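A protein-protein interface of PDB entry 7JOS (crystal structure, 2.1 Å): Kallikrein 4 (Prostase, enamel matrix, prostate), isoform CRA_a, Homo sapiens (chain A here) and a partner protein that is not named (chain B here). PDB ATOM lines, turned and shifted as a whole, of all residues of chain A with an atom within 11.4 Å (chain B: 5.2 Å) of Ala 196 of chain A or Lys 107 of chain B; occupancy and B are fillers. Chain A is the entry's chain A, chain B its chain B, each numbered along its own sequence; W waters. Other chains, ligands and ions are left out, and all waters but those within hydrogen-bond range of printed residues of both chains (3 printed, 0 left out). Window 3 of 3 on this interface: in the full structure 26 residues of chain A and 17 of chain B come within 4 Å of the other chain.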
ATOM      1  N   ILE A   2       1.750   2.223  13.795  1.00  0.00           N
ATOM      2  CA  ILE A   2       3.230   2.029  13.796  1.00  0.00           C
ATOM      3  C   ILE A   2       3.676   1.639  12.382  1.00  0.00           C
ATOM      4  O   ILE A   2       3.169   0.619  11.868  1.00  0.00           O
ATOM      5  CB  ILE A   2       3.641   0.939  14.813  1.00  0.00           C
ATOM      6  CG1 ILE A   2       3.070   1.166  16.212  1.00  0.00           C
ATOM      7  CG2 ILE A   2       5.165   0.813  14.852  1.00  0.00           C
ATOM      8  CD1 ILE A   2       3.498   2.486  16.841  1.00  0.00           C
ATOM      9  N   LEU A  83     -11.926  -8.533  28.297  1.00  0.00           N
ATOM     10  CA  LEU A  83     -11.445  -7.995  27.006  1.00  0.00           C
ATOM     11  C   LEU A  83     -12.303  -8.467  25.831  1.00  0.00           C
ATOM     12  O   LEU A  83     -12.142  -7.898  24.724  1.00  0.00           O
ATOM     13  CB  LEU A  83      -9.986  -8.388  26.783  1.00  0.00           C
ATOM     14  CG  LEU A  83      -8.986  -7.910  27.827  1.00  0.00           C
ATOM     15  CD1 LEU A  83      -7.575  -8.183  27.329  1.00  0.00           C
ATOM     16  CD2 LEU A  83      -9.158  -6.424  28.102  1.00  0.00           C
ATOM     17  N   LEU A 125      -0.649   6.801  18.202  1.00  0.00           N
ATOM     18  CA  LEU A 125       0.807   7.092  18.263  1.00  0.00           C
ATOM     19  C   LEU A 125       1.546   6.463  17.086  1.00  0.00           C
ATOM     20  O   LEU A 125       1.159   5.371  16.646  1.00  0.00           O
ATOM     21  CB  LEU A 125       1.388   6.542  19.563  1.00  0.00           C
ATOM     22  CG  LEU A 125       0.895   7.176  20.858  1.00  0.00           C
ATOM     23  CD1 LEU A 125       1.559   6.500  22.055  1.00  0.00           C
ATOM     24  CD2 LEU A 125       1.185   8.663  20.870  1.00  0.00           C
ATOM     25  N   LEU A 151      -0.379 -16.637  21.684  1.00  0.00           N
ATOM     26  CA  LEU A 151       0.257 -15.385  22.146  1.00  0.00           C
ATOM     27  C   LEU A 151      -0.538 -14.710  23.258  1.00  0.00           C
ATOM     28  O   LEU A 151       0.059 -13.994  24.060  1.00  0.00           O
ATOM     29  CB  LEU A 151       0.357 -14.443  20.945  1.00  0.00           C
ATOM     30  CG  LEU A 151       1.747 -13.909  20.661  1.00  0.00           C
ATOM     31  CD1 LEU A 151       2.684 -15.006  20.169  1.00  0.00           C
ATOM     32  CD2 LEU A 151       1.603 -12.849  19.622  1.00  0.00           C
ATOM     33  N   TYR A 152      -1.862 -14.903  23.314  1.00  0.00           N
ATOM     34  CA  TYR A 152      -2.699 -14.056  24.211  1.00  0.00           C
ATOM     35  C   TYR A 152      -3.373 -14.883  25.308  1.00  0.00           C
ATOM     36  O   TYR A 152      -4.227 -14.387  26.061  1.00  0.00           O
ATOM     37  CB  TYR A 152      -3.672 -13.236  23.375  1.00  0.00           C
ATOM     38  CG  TYR A 152      -3.023 -12.030  22.734  1.00  0.00           C
ATOM     39  CD1 TYR A 152      -2.655 -10.924  23.478  1.00  0.00           C
ATOM     40  CD2 TYR A 152      -2.716 -12.016  21.374  1.00  0.00           C
ATOM     41  CE1 TYR A 152      -2.029  -9.840  22.893  1.00  0.00           C
ATOM     42  CE2 TYR A 152      -2.070 -10.955  20.789  1.00  0.00           C
ATOM     43  CZ  TYR A 152      -1.738  -9.851  21.548  1.00  0.00           C
ATOM     44  OH  TYR A 152      -1.118  -8.796  20.961  1.00  0.00           O
ATOM     45  N   ASP A 153      -3.033 -16.182  25.338  1.00  0.00           N
ATOM     46  CA  ASP A 153      -3.364 -17.079  26.482  1.00  0.00           C
ATOM     47  C   ASP A 153      -3.093 -16.360  27.791  1.00  0.00           C
ATOM     48  O   ASP A 153      -2.054 -15.720  27.900  1.00  0.00           O
ATOM     49  CB  ASP A 153      -2.360 -18.234  26.415  1.00  0.00           C
ATOM     50  CG  ASP A 153      -2.498 -19.385  27.394  1.00  0.00           C
ATOM     51  OD1 ASP A 153      -3.384 -19.394  28.238  1.00  0.00           O
ATOM     52  OD2 ASP A 153      -1.704 -20.287  27.240  1.00  0.00           O
ATOM     53  N   PRO A 154      -3.944 -16.460  28.830  1.00  0.00           N
ATOM     54  CA  PRO A 154      -5.186 -17.230  28.801  1.00  0.00           C
ATOM     55  C   PRO A 154      -6.455 -16.450  28.404  1.00  0.00           C
ATOM     56  O   PRO A 154      -7.541 -16.881  28.732  1.00  0.00           O
ATOM     57  CB  PRO A 154      -5.267 -17.655  30.279  1.00  0.00           C
ATOM     58  CG  PRO A 154      -4.796 -16.429  31.017  1.00  0.00           C
ATOM     59  CD  PRO A 154      -3.695 -15.865  30.145  1.00  0.00           C
ATOM     60  N   LEU A 155      -6.304 -15.304  27.747  1.00  0.00           N
ATOM     61  CA  LEU A 155      -7.462 -14.396  27.523  1.00  0.00           C
ATOM     62  C   LEU A 155      -8.104 -14.535  26.125  1.00  0.00           C
ATOM     63  O   LEU A 155      -9.088 -13.749  25.792  1.00  0.00           O
ATOM     64  CB  LEU A 155      -6.966 -12.972  27.778  1.00  0.00           C
ATOM     65  CG  LEU A 155      -6.671 -12.694  29.258  1.00  0.00           C
ATOM     66  CD1 LEU A 155      -5.988 -11.365  29.424  1.00  0.00           C
ATOM     67  CD2 LEU A 155      -7.928 -12.755  30.136  1.00  0.00           C
ATOM     68  N   GLN A 169       7.218  -4.873  11.485  1.00  0.00           N
ATOM     69  CA  GLN A 169       6.755  -4.252  12.764  1.00  0.00           C
ATOM     70  C   GLN A 169       5.594  -3.267  12.542  1.00  0.00           C
ATOM     71  O   GLN A 169       5.613  -2.169  13.103  1.00  0.00           O
ATOM     72  CB  GLN A 169       7.923  -3.559  13.452  1.00  0.00           C
ATOM     73  CG  GLN A 169       8.973  -4.538  13.937  1.00  0.00           C
ATOM     74  CD  GLN A 169      10.046  -3.793  14.688  1.00  0.00           C
ATOM     75  OE1 GLN A 169      11.101  -3.494  14.147  1.00  0.00           O
ATOM     76  NE2 GLN A 169       9.747  -3.426  15.921  1.00  0.00           N
ATOM     77  N   ASP A 171       1.753  -2.153  13.185  1.00  0.00           N
ATOM     78  CA  ASP A 171       0.802  -2.447  14.289  1.00  0.00           C
ATOM     79  C   ASP A 171      -0.101  -1.222  14.478  1.00  0.00           C
ATOM     80  O   ASP A 171       0.183  -0.139  13.881  1.00  0.00           O
ATOM     81  CB  ASP A 171       1.510  -2.825  15.604  1.00  0.00           C
ATOM     82  CG  ASP A 171       0.659  -3.588  16.644  1.00  0.00           C
ATOM     83  OD1 ASP A 171      -0.529  -3.922  16.345  1.00  0.00           O
ATOM     84  OD2 ASP A 171       1.176  -3.871  17.776  1.00  0.00           O
ATOM     85  N   SER A 172      -1.155  -1.430  15.263  1.00  0.00           N
ATOM     86  CA  SER A 172      -1.976  -0.340  15.832  1.00  0.00           C
ATOM     87  C   SER A 172      -1.324   0.105  17.144  1.00  0.00           C
ATOM     88  O   SER A 172      -0.487  -0.619  17.684  1.00  0.00           O
ATOM     89  CB  SER A 172      -3.414  -0.794  16.003  1.00  0.00           C
ATOM     90  OG  SER A 172      -3.453  -2.054  16.666  1.00  0.00           O
ATOM     91  N   CYS A 173      -1.669   1.299  17.609  1.00  0.00           N
ATOM     92  CA  CYS A 173      -1.063   1.789  18.867  1.00  0.00           C
ATOM     93  C   CYS A 173      -2.087   2.657  19.596  1.00  0.00           C
ATOM     94  O   CYS A 173      -3.221   2.789  19.109  1.00  0.00           O
ATOM     95  CB  CYS A 173       0.254   2.513  18.596  1.00  0.00           C
ATOM     96  SG  CYS A 173       1.290   2.671  20.089  1.00  0.00           S
ATOM     97  N   ASN A 174      -1.684   3.235  20.715  1.00  0.00           N
ATOM     98  CA  ASN A 174      -2.585   3.974  21.619  1.00  0.00           C
ATOM     99  C   ASN A 174      -3.192   5.179  20.891  1.00  0.00           C
ATOM    100  O   ASN A 174      -2.448   5.958  20.312  1.00  0.00           O
ATOM    101  CB  ASN A 174      -1.844   4.331  22.905  1.00  0.00           C
ATOM    102  CG  ASN A 174      -1.510   3.107  23.734  1.00  0.00           C
ATOM    103  OD1 ASN A 174      -1.954   2.001  23.432  1.00  0.00           O
ATOM    104  ND2 ASN A 174      -0.732   3.288  24.777  1.00  0.00           N
ATOM    105  N   SER A 192      -8.639  -3.215  19.108  1.00  0.00           N
ATOM    106  CA  SER A 192      -9.109  -3.499  20.486  1.00  0.00           C
ATOM    107  C   SER A 192      -7.922  -3.411  21.446  1.00  0.00           C
ATOM    108  O   SER A 192      -7.847  -2.442  22.215  1.00  0.00           O
ATOM    109  CB  SER A 192      -9.822  -4.836  20.529  1.00  0.00           C
ATOM    110  OG  SER A 192     -10.246  -5.152  21.848  1.00  0.00           O
ATOM    111  N   PHE A 193      -6.978  -4.344  21.353  1.00  0.00           N
ATOM    112  CA  PHE A 193      -5.867  -4.324  22.330  1.00  0.00           C
ATOM    113  C   PHE A 193      -4.682  -5.078  21.760  1.00  0.00           C
ATOM    114  O   PHE A 193      -4.782  -5.673  20.674  1.00  0.00           O
ATOM    115  CB  PHE A 193      -6.308  -4.941  23.655  1.00  0.00           C
ATOM    116  CG  PHE A 193      -6.541  -6.428  23.637  1.00  0.00           C
ATOM    117  CD1 PHE A 193      -7.795  -6.944  23.387  1.00  0.00           C
ATOM    118  CD2 PHE A 193      -5.516  -7.302  23.962  1.00  0.00           C
ATOM    119  CE1 PHE A 193      -8.016  -8.319  23.406  1.00  0.00           C
ATOM    120  CE2 PHE A 193      -5.746  -8.668  24.011  1.00  0.00           C
ATOM    121  CZ  PHE A 193      -6.981  -9.177  23.717  1.00  0.00           C
ATOM    122  N   GLY A 194      -3.579  -5.001  22.492  1.00  0.00           N
ATOM    123  CA  GLY A 194      -2.372  -5.756  22.161  1.00  0.00           C
ATOM    124  C   GLY A 194      -1.362  -5.670  23.292  1.00  0.00           C
ATOM    125  O   GLY A 194      -1.669  -5.102  24.336  1.00  0.00           O
ATOM    126  N   LYS A 195      -0.170  -6.177  23.041  1.00  0.00           N
ATOM    127  CA  LYS A 195       0.913  -6.102  24.043  1.00  0.00           C
ATOM    128  C   LYS A 195       1.468  -4.683  24.038  1.00  0.00           C
ATOM    129  O   LYS A 195       1.518  -4.064  22.937  1.00  0.00           O
ATOM    130  CB  LYS A 195       1.957  -7.177  23.732  1.00  0.00           C
ATOM    131  CG  LYS A 195       1.418  -8.561  24.022  1.00  0.00           C
ATOM    132  CD  LYS A 195       2.402  -9.674  24.035  1.00  0.00           C
ATOM    133  CE  LYS A 195       1.692 -10.999  24.162  1.00  0.00           C
ATOM    134  NZ  LYS A 195       2.714 -12.067  24.272  1.00  0.00           N
ATOM    135  N   ALA A 196       1.786  -4.194  25.244  1.00  0.00           N
ATOM    136  CA  ALA A 196       2.530  -2.932  25.458  1.00  0.00           C
ATOM    137  C   ALA A 196       3.996  -3.283  25.694  1.00  0.00           C
ATOM    138  O   ALA A 196       4.276  -4.125  26.538  1.00  0.00           O
ATOM    139  CB  ALA A 196       1.919  -2.219  26.637  1.00  0.00           C
ATOM    140  N   PRO A 197       4.973  -2.711  24.951  1.00  0.00           N
ATOM    141  CA  PRO A 197       4.729  -1.683  23.937  1.00  0.00           C
ATOM    142  C   PRO A 197       4.275  -2.218  22.568  1.00  0.00           C
ATOM    143  O   PRO A 197       4.433  -3.398  22.298  1.00  0.00           O
ATOM    144  CB  PRO A 197       6.132  -1.078  23.779  1.00  0.00           C
ATOM    145  CG  PRO A 197       7.049  -2.278  23.918  1.00  0.00           C
ATOM    146  CD  PRO A 197       6.399  -3.067  25.039  1.00  0.00           C
ATOM    147  N   CYS A 198       3.783  -1.319  21.707  1.00  0.00           N
ATOM    148  CA  CYS A 198       3.268  -1.690  20.368  1.00  0.00           C
ATOM    149  C   CYS A 198       4.417  -1.959  19.417  1.00  0.00           C
ATOM    150  O   CYS A 198       5.488  -1.451  19.651  1.00  0.00           O
ATOM    151  CB  CYS A 198       2.420  -0.573  19.782  1.00  0.00           C
ATOM    152  SG  CYS A 198       1.214  -0.016  20.997  1.00  0.00           S
ATOM    153  N   GLY A 199       4.136  -2.696  18.351  1.00  0.00           N
ATOM    154  CA  GLY A 199       5.090  -2.862  17.248  1.00  0.00           C
ATOM    155  C   GLY A 199       6.141  -3.929  17.525  1.00  0.00           C
ATOM    156  O   GLY A 199       7.030  -4.062  16.641  1.00  0.00           O
ATOM    157  N   GLN A 200       6.055  -4.694  18.627  1.00  0.00           N
ATOM    158  CA  GLN A 200       7.088  -5.742  18.878  1.00  0.00           C
ATOM    159  C   GLN A 200       7.102  -6.730  17.708  1.00  0.00           C
ATOM    160  O   GLN A 200       6.014  -7.046  17.176  1.00  0.00           O
ATOM    161  CB  GLN A 200       6.861  -6.469  20.201  1.00  0.00           C
ATOM    162  CG  GLN A 200       6.646  -5.558  21.412  1.00  0.00           C
ATOM    163  CD  GLN A 200       6.394  -6.338  22.678  1.00  0.00           C
ATOM    164  OE1 GLN A 200       6.954  -7.415  22.865  1.00  0.00           O
ATOM    165  NE2 GLN A 200       5.573  -5.801  23.584  1.00  0.00           N
ATOM    166  N   VAL A 201       8.287  -7.194  17.298  1.00  0.00           N
ATOM    167  CA  VAL A 201       8.412  -8.122  16.126  1.00  0.00           C
ATOM    168  C   VAL A 201       7.677  -9.420  16.477  1.00  0.00           C
ATOM    169  O   VAL A 201       7.774  -9.846  17.643  1.00  0.00           O
ATOM    170  CB  VAL A 201       9.886  -8.437  15.782  1.00  0.00           C
ATOM    171  CG1 VAL A 201      10.002  -9.099  14.414  1.00  0.00           C
ATOM    172  CG2 VAL A 201      10.801  -7.221  15.895  1.00  0.00           C
ATOM    173  N   VAL A 203       4.687  -9.905  17.155  1.00  0.00           N
ATOM    174  CA  VAL A 203       3.510  -9.740  18.069  1.00  0.00           C
ATOM    175  C   VAL A 203       2.343  -9.043  17.359  1.00  0.00           C
ATOM    176  O   VAL A 203       2.277  -7.824  17.273  1.00  0.00           O
ATOM    177  CB  VAL A 203       3.906  -9.022  19.364  1.00  0.00           C
ATOM    178  CG1 VAL A 203       2.741  -8.900  20.345  1.00  0.00           C
ATOM    179  CG2 VAL A 203       5.097  -9.731  20.018  1.00  0.00           C
ATOM    180  N   PRO A 204       1.360  -9.786  16.815  1.00  0.00           N
ATOM    181  CA  PRO A 204       0.187  -9.166  16.219  1.00  0.00           C
ATOM    182  C   PRO A 204      -0.711  -8.508  17.278  1.00  0.00           C
ATOM    183  O   PRO A 204      -0.663  -8.873  18.425  1.00  0.00           O
ATOM    184  CB  PRO A 204      -0.536 -10.329  15.521  1.00  0.00           C
ATOM    185  CG  PRO A 204      -0.123 -11.540  16.316  1.00  0.00           C
ATOM    186  CD  PRO A 204       1.314 -11.252  16.701  1.00  0.00           C
ATOM    187  N   GLY A 205      -1.474  -7.515  16.839  1.00  0.00           N
ATOM    188  CA  GLY A 205      -2.510  -6.853  17.652  1.00  0.00           C
ATOM    189  C   GLY A 205      -3.810  -7.614  17.594  1.00  0.00           C
ATOM    190  O   GLY A 205      -3.943  -8.495  16.712  1.00  0.00           O
ATOM    191  N   VAL A 206      -4.708  -7.300  18.523  1.00  0.00           N
ATOM    192  CA  VAL A 206      -6.021  -7.982  18.619  1.00  0.00           C
ATOM    193  C   VAL A 206      -7.116  -7.021  18.178  1.00  0.00           C
ATOM    194  O   VAL A 206      -7.077  -5.833  18.551  1.00  0.00           O
ATOM    195  CB  VAL A 206      -6.281  -8.526  20.024  1.00  0.00           C
ATOM    196  CG1 VAL A 206      -7.548  -9.377  20.061  1.00  0.00           C
ATOM    197  CG2 VAL A 206      -5.093  -9.337  20.496  1.00  0.00           C
ATOM    198  N   GLU B  61      -0.558   0.914  32.977  1.00  0.00           N
ATOM    199  CA  GLU B  61      -0.539   0.248  31.644  1.00  0.00           C
ATOM    200  C   GLU B  61      -1.759  -0.654  31.477  1.00  0.00           C
ATOM    201  O   GLU B  61      -1.941  -1.575  32.312  1.00  0.00           O
ATOM    202  CB  GLU B  61       0.693  -0.634  31.519  1.00  0.00           C
ATOM    203  CG  GLU B  61       1.763  -0.115  30.616  1.00  0.00           C
ATOM    204  CD  GLU B  61       2.875  -1.150  30.400  1.00  0.00           C
ATOM    205  OE1 GLU B  61       2.595  -2.406  30.378  1.00  0.00           O
ATOM    206  OE2 GLU B  61       4.029  -0.709  30.300  1.00  0.00           O
ATOM    207  N   SER B  62      -2.494  -0.421  30.389  1.00  0.00           N
ATOM    208  CA  SER B  62      -3.560  -1.322  29.908  1.00  0.00           C
ATOM    209  C   SER B  62      -3.180  -1.792  28.518  1.00  0.00           C
ATOM    210  O   SER B  62      -2.671  -1.007  27.719  1.00  0.00           O
ATOM    211  CB  SER B  62      -4.882  -0.573  29.855  1.00  0.00           C
ATOM    212  OG  SER B  62      -5.871  -1.345  29.208  1.00  0.00           O
ATOM    213  N   ARG B  65      -5.897  -0.302  23.273  1.00  0.00           N
ATOM    214  CA  ARG B  65      -5.166   0.674  22.422  1.00  0.00           C
ATOM    215  C   ARG B  65      -5.746   2.085  22.576  1.00  0.00           C
ATOM    216  O   ARG B  65      -5.837   2.804  21.565  1.00  0.00           O
ATOM    217  CB  ARG B  65      -5.197   0.225  20.955  1.00  0.00           C
ATOM    218  CG  ARG B  65      -4.424  -1.045  20.673  1.00  0.00           C
ATOM    219  CD  ARG B  65      -3.069  -1.022  21.310  1.00  0.00           C
ATOM    220  NE  ARG B  65      -2.110  -1.897  20.655  1.00  0.00           N
ATOM    221  CZ  ARG B  65      -1.150  -2.540  21.299  1.00  0.00           C
ATOM    222  NH1 ARG B  65      -1.019  -2.425  22.627  1.00  0.00           N
ATOM    223  NH2 ARG B  65      -0.340  -3.314  20.603  1.00  0.00           N
ATOM    224  N   ASN B  76      -1.546  -2.866  34.853  1.00  0.00           N
ATOM    225  CA  ASN B  76      -0.225  -3.040  35.494  1.00  0.00           C
ATOM    226  C   ASN B  76       0.213  -1.670  36.003  1.00  0.00           C
ATOM    227  O   ASN B  76      -0.093  -0.634  35.360  1.00  0.00           O
ATOM    228  CB  ASN B  76       0.800  -3.647  34.546  1.00  0.00           C
ATOM    229  CG  ASN B  76       0.607  -5.137  34.403  1.00  0.00           C
ATOM    230  OD1 ASN B  76       0.700  -5.854  35.403  1.00  0.00           O
ATOM    231  ND2 ASN B  76       0.347  -5.606  33.190  1.00  0.00           N
ATOM    232  N   LYS B  78       3.812   0.177  37.327  1.00  0.00           N
ATOM    233  CA  LYS B  78       5.255  -0.173  37.316  1.00  0.00           C
ATOM    234  C   LYS B  78       6.107   1.080  37.497  1.00  0.00           C
ATOM    235  O   LYS B  78       5.695   2.202  37.094  1.00  0.00           O
ATOM    236  CB  LYS B  78       5.620  -0.937  36.049  1.00  0.00           C
ATOM    237  CG  LYS B  78       5.733  -0.108  34.793  1.00  0.00           C
ATOM    238  CD  LYS B  78       6.140  -0.971  33.602  1.00  0.00           C
ATOM    239  CE  LYS B  78       6.243  -0.182  32.314  1.00  0.00           C
ATOM    240  NZ  LYS B  78       6.411  -1.089  31.158  1.00  0.00           N
ATOM    241  N   ASP B  85      10.343  -3.907  32.019  1.00  0.00           N
ATOM    242  CA  ASP B  85       9.342  -4.663  32.826  1.00  0.00           C
ATOM    243  C   ASP B  85      10.009  -5.212  34.096  1.00  0.00           C
ATOM    244  O   ASP B  85       9.553  -6.247  34.603  1.00  0.00           O
ATOM    245  CB  ASP B  85       8.699  -5.821  32.049  1.00  0.00           C
ATOM    246  CG  ASP B  85       7.621  -5.425  31.059  1.00  0.00           C
ATOM    247  OD1 ASP B  85       7.129  -4.279  31.145  1.00  0.00           O
ATOM    248  OD2 ASP B  85       7.260  -6.275  30.224  1.00  0.00           O
ATOM    249  N   VAL B  88       7.642  -4.052  37.871  1.00  0.00           N
ATOM    250  CA  VAL B  88       6.173  -4.301  37.786  1.00  0.00           C
ATOM    251  C   VAL B  88       5.629  -4.714  39.156  1.00  0.00           C
ATOM    252  O   VAL B  88       6.134  -5.667  39.756  1.00  0.00           O
ATOM    253  CB  VAL B  88       5.869  -5.367  36.719  1.00  0.00           C
ATOM    254  CG1 VAL B  88       4.403  -5.754  36.716  1.00  0.00           C
ATOM    255  CG2 VAL B  88       6.299  -4.886  35.351  1.00  0.00           C
ATOM    256  N   ASP B 105       9.936  -8.837  37.860  1.00  0.00           N
ATOM    257  CA  ASP B 105      10.467  -8.522  36.505  1.00  0.00           C
ATOM    258  C   ASP B 105       9.610  -9.240  35.457  1.00  0.00           C
ATOM    259  O   ASP B 105      10.010  -9.242  34.301  1.00  0.00           O
ATOM    260  CB  ASP B 105      11.957  -8.858  36.413  1.00  0.00           C
ATOM    261  CG  ASP B 105      12.281 -10.305  36.742  1.00  0.00           C
ATOM    262  OD1 ASP B 105      11.321 -11.126  36.980  1.00  0.00           O
ATOM    263  OD2 ASP B 105      13.506 -10.592  36.815  1.00  0.00           O
ATOM    264  N   THR B 106       8.475  -9.807  35.870  1.00  0.00           N
ATOM    265  CA  THR B 106       7.515 -10.437  34.924  1.00  0.00           C
ATOM    266  C   THR B 106       6.213  -9.627  34.933  1.00  0.00           C
ATOM    267  O   THR B 106       5.865  -9.031  35.951  1.00  0.00           O
ATOM    268  CB  THR B 106       7.263 -11.908  35.296  1.00  0.00           C
ATOM    269  OG1 THR B 106       6.618 -11.905  36.574  1.00  0.00           O
ATOM    270  CG2 THR B 106       8.529 -12.734  35.379  1.00  0.00           C
ATOM    271  N   LYS B 107       5.484  -9.682  33.829  1.00  0.00           N
ATOM    272  CA  LYS B 107       4.246  -8.896  33.627  1.00  0.00           C
ATOM    273  C   LYS B 107       3.225  -9.772  32.893  1.00  0.00           C
ATOM    274  O   LYS B 107       3.585 -10.323  31.885  1.00  0.00           O
ATOM    275  CB  LYS B 107       4.622  -7.679  32.791  1.00  0.00           C
ATOM    276  CG  LYS B 107       3.515  -6.667  32.613  1.00  0.00           C
ATOM    277  CD  LYS B 107       3.943  -5.435  31.888  1.00  0.00           C
ATOM    278  CE  LYS B 107       3.938  -5.594  30.393  1.00  0.00           C
ATOM    279  NZ  LYS B 107       4.363  -4.320  29.762  1.00  0.00           N
ATOM    280  N   SER B 108       2.023  -9.930  33.434  1.00  0.00           N
ATOM    281  CA  SER B 108       0.883 -10.467  32.654  1.00  0.00           C
ATOM    282  C   SER B 108       0.386  -9.399  31.670  1.00  0.00           C
ATOM    283  O   SER B 108       0.600  -8.202  31.904  1.00  0.00           O
ATOM    284  CB  SER B 108      -0.249 -10.873  33.548  1.00  0.00           C
ATOM    285  OG  SER B 108       0.193 -11.831  34.485  1.00  0.00           O
ATOM    286  N   LEU B 109      -0.302  -9.840  30.628  1.00  0.00           N
ATOM    287  CA  LEU B 109      -0.918  -8.938  29.624  1.00  0.00           C
ATOM    288  C   LEU B 109      -1.861  -7.955  30.334  1.00  0.00           C
ATOM    289  O   LEU B 109      -1.832  -6.767  30.014  1.00  0.00           O
ATOM    290  CB  LEU B 109      -1.707  -9.835  28.671  1.00  0.00           C
ATOM    291  CG  LEU B 109      -2.568  -9.106  27.652  1.00  0.00           C
ATOM    292  CD1 LEU B 109      -1.678  -8.539  26.555  1.00  0.00           C
ATOM    293  CD2 LEU B 109      -3.626 -10.067  27.121  1.00  0.00           C
HETATM  294  O   HOH W   1      -1.884  -0.472  24.968  1.00  0.00           O
HETATM  295  O   HOH W   2      -2.224  -3.479  18.560  1.00  0.00           O
HETATM  296  O   HOH W   3       0.965  -5.937  19.487  1.00  0.00           O
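The guanidinium group of Arg 65 of chain B sits close to the side-chain sulfur of Cys 198 of chain A, at 3.7 Å.
N of Arg 65 of chain B sits at hydrogen-bond distance from O of Ser 192 of chain A, at 3.1 Å.
The side-chain carboxylate (OD2) of Asp 171 of chain A is in salt-bridge range of the guanidinium group (NH2) of Arg 65 of chain B.
O of Lys 195 of chain A sits at hydrogen-bond distance from NH1 of Arg 65 of chain B (3.0 Å).
The guanidinium group (NH1) of Arg 65 of chain B is in hydrogen-bond range of the backbone carbonyl oxygen (O) of Gly 194 of chain A, at 3.2 Å.
NZ of Lys 107 of chain B sits at hydrogen-bond distance from O of Ala 196 of chain A (3.2 Å).
O of Leu 151 of chain A is in hydrogen-bond range of NZ of Lys 195 of chain A.
N of Gly 199 of chain A lies within hydrogen-bond range of OD2 of Asp 171 of chain A.
N of Val 206 of chain A sits at hydrogen-bond distance from O of Phe 193 of chain A (2.7 Å).
The backbone NH of Asn 76 of chain B is in hydrogen-bond range of the backbone carbonyl oxygen of Glu 61 of chain B (2.9 Å).
The backbone NH (N) of Ser 192 of chain A sits at hydrogen-bond distance from the backbone carbonyl oxygen (O) of Val 206 of chain A (3.1 Å).
The side-chain hydroxyl (OH) of Tyr 152 of chain A lies within hydrogen-bond range of the backbone carbonyl oxygen (O) of Pro 204 of chain A, at 2.6 Å.
Among the printed residues, merely in contact across the chains: Tyr 152 of chain A with Leu 109 of chain B (3.9 Å), Leu 155 of chain A with Leu 109 of chain B (3.5 Å), Ser 172 of chain A with Arg 65 of chain B (3.6 Å), Cys 173 of chain A with Arg 65 of chain B (3.6 Å), Asn 174 of chain A with Arg 65 of chain B (3.5 Å), Phe 193 of chain A with Arg 65 of chain B (3.9 Å) and Ala 196 of chain A with Glu 61 of chain B (3.8 Å).
Of the printed residues of chain B, Ala 196 of chain A touches Glu 61 and Lys 107.
Lys 107 of chain B touches just one residue of chain A: Ala 196.
No residue of chain A comes within 4 Å of Asn 76 of chain B.
No residue of chain A comes within 4 Å of Asp 85 of chain B.
No residue of chain A comes within 4 Å of Val 88 of chain B.
No residue of chain A comes within 4 Å of Thr 106 of chain B.
No residue of chain A comes within 4 Å of Ser 108 of chain B.
Of the printed residues of chain B, Tyr 152 of chain A touches Leu 109.
Printed residues of chain A within 4 Å of Leu 109 of chain B: Tyr 152 and Leu 155.
Val 201 of chain A touches none of the printed residues of chain B.
Leu 125 of chain A touches none of the printed residues of chain B.
The nearest printed residue of chain B that does not touch Asn 174 of chain A is Ser 62 of chain B (5.3 Å).
Of the 27 printed residues of chain A, 12 touch a printed residue of chain B.
Hydrophobic or aromatic side chains of chain A that line the printed part of chain B: Tyr 152, Leu 155 and Ala 196.
Along chain A the printed residues that touch a printed residue of chain B span positions 152 to 198.
Among the printed residues, 13 pairs touch across the chains.
Among the printed residues, Asp or Glu carboxylates within 4 Å of a Lys or Arg side-chain nitrogen of the other chain: Asp 171 of chain A with Arg 65 of chain B (3.3 Å).
Water W2 lies within hydrogen-bond range of NE of Arg 65 of chain B (2.6 Å), OG of Ser 172 of chain A (2.7 Å) and OD1 of Asp 171 of chain A (2.8 Å).
Water W3 lies within hydrogen-bond range of the side-chain carboxylate (OD2) of Asp 171 of chain A (2.7 Å), the guanidinium group (NH2) of Arg 65 of chain B (3.1 Å) and the backbone carbonyl oxygen (O) of Val 203 of chain A (3.2 Å).
Water W1 lies within hydrogen-bond range of the backbone carbonyl oxygen (O) of Ser 62 of chain B, the side-chain amide oxygen (OD1) of Asn 174 of chain A and the guanidinium group (NH1) of Arg 65 of chain B.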
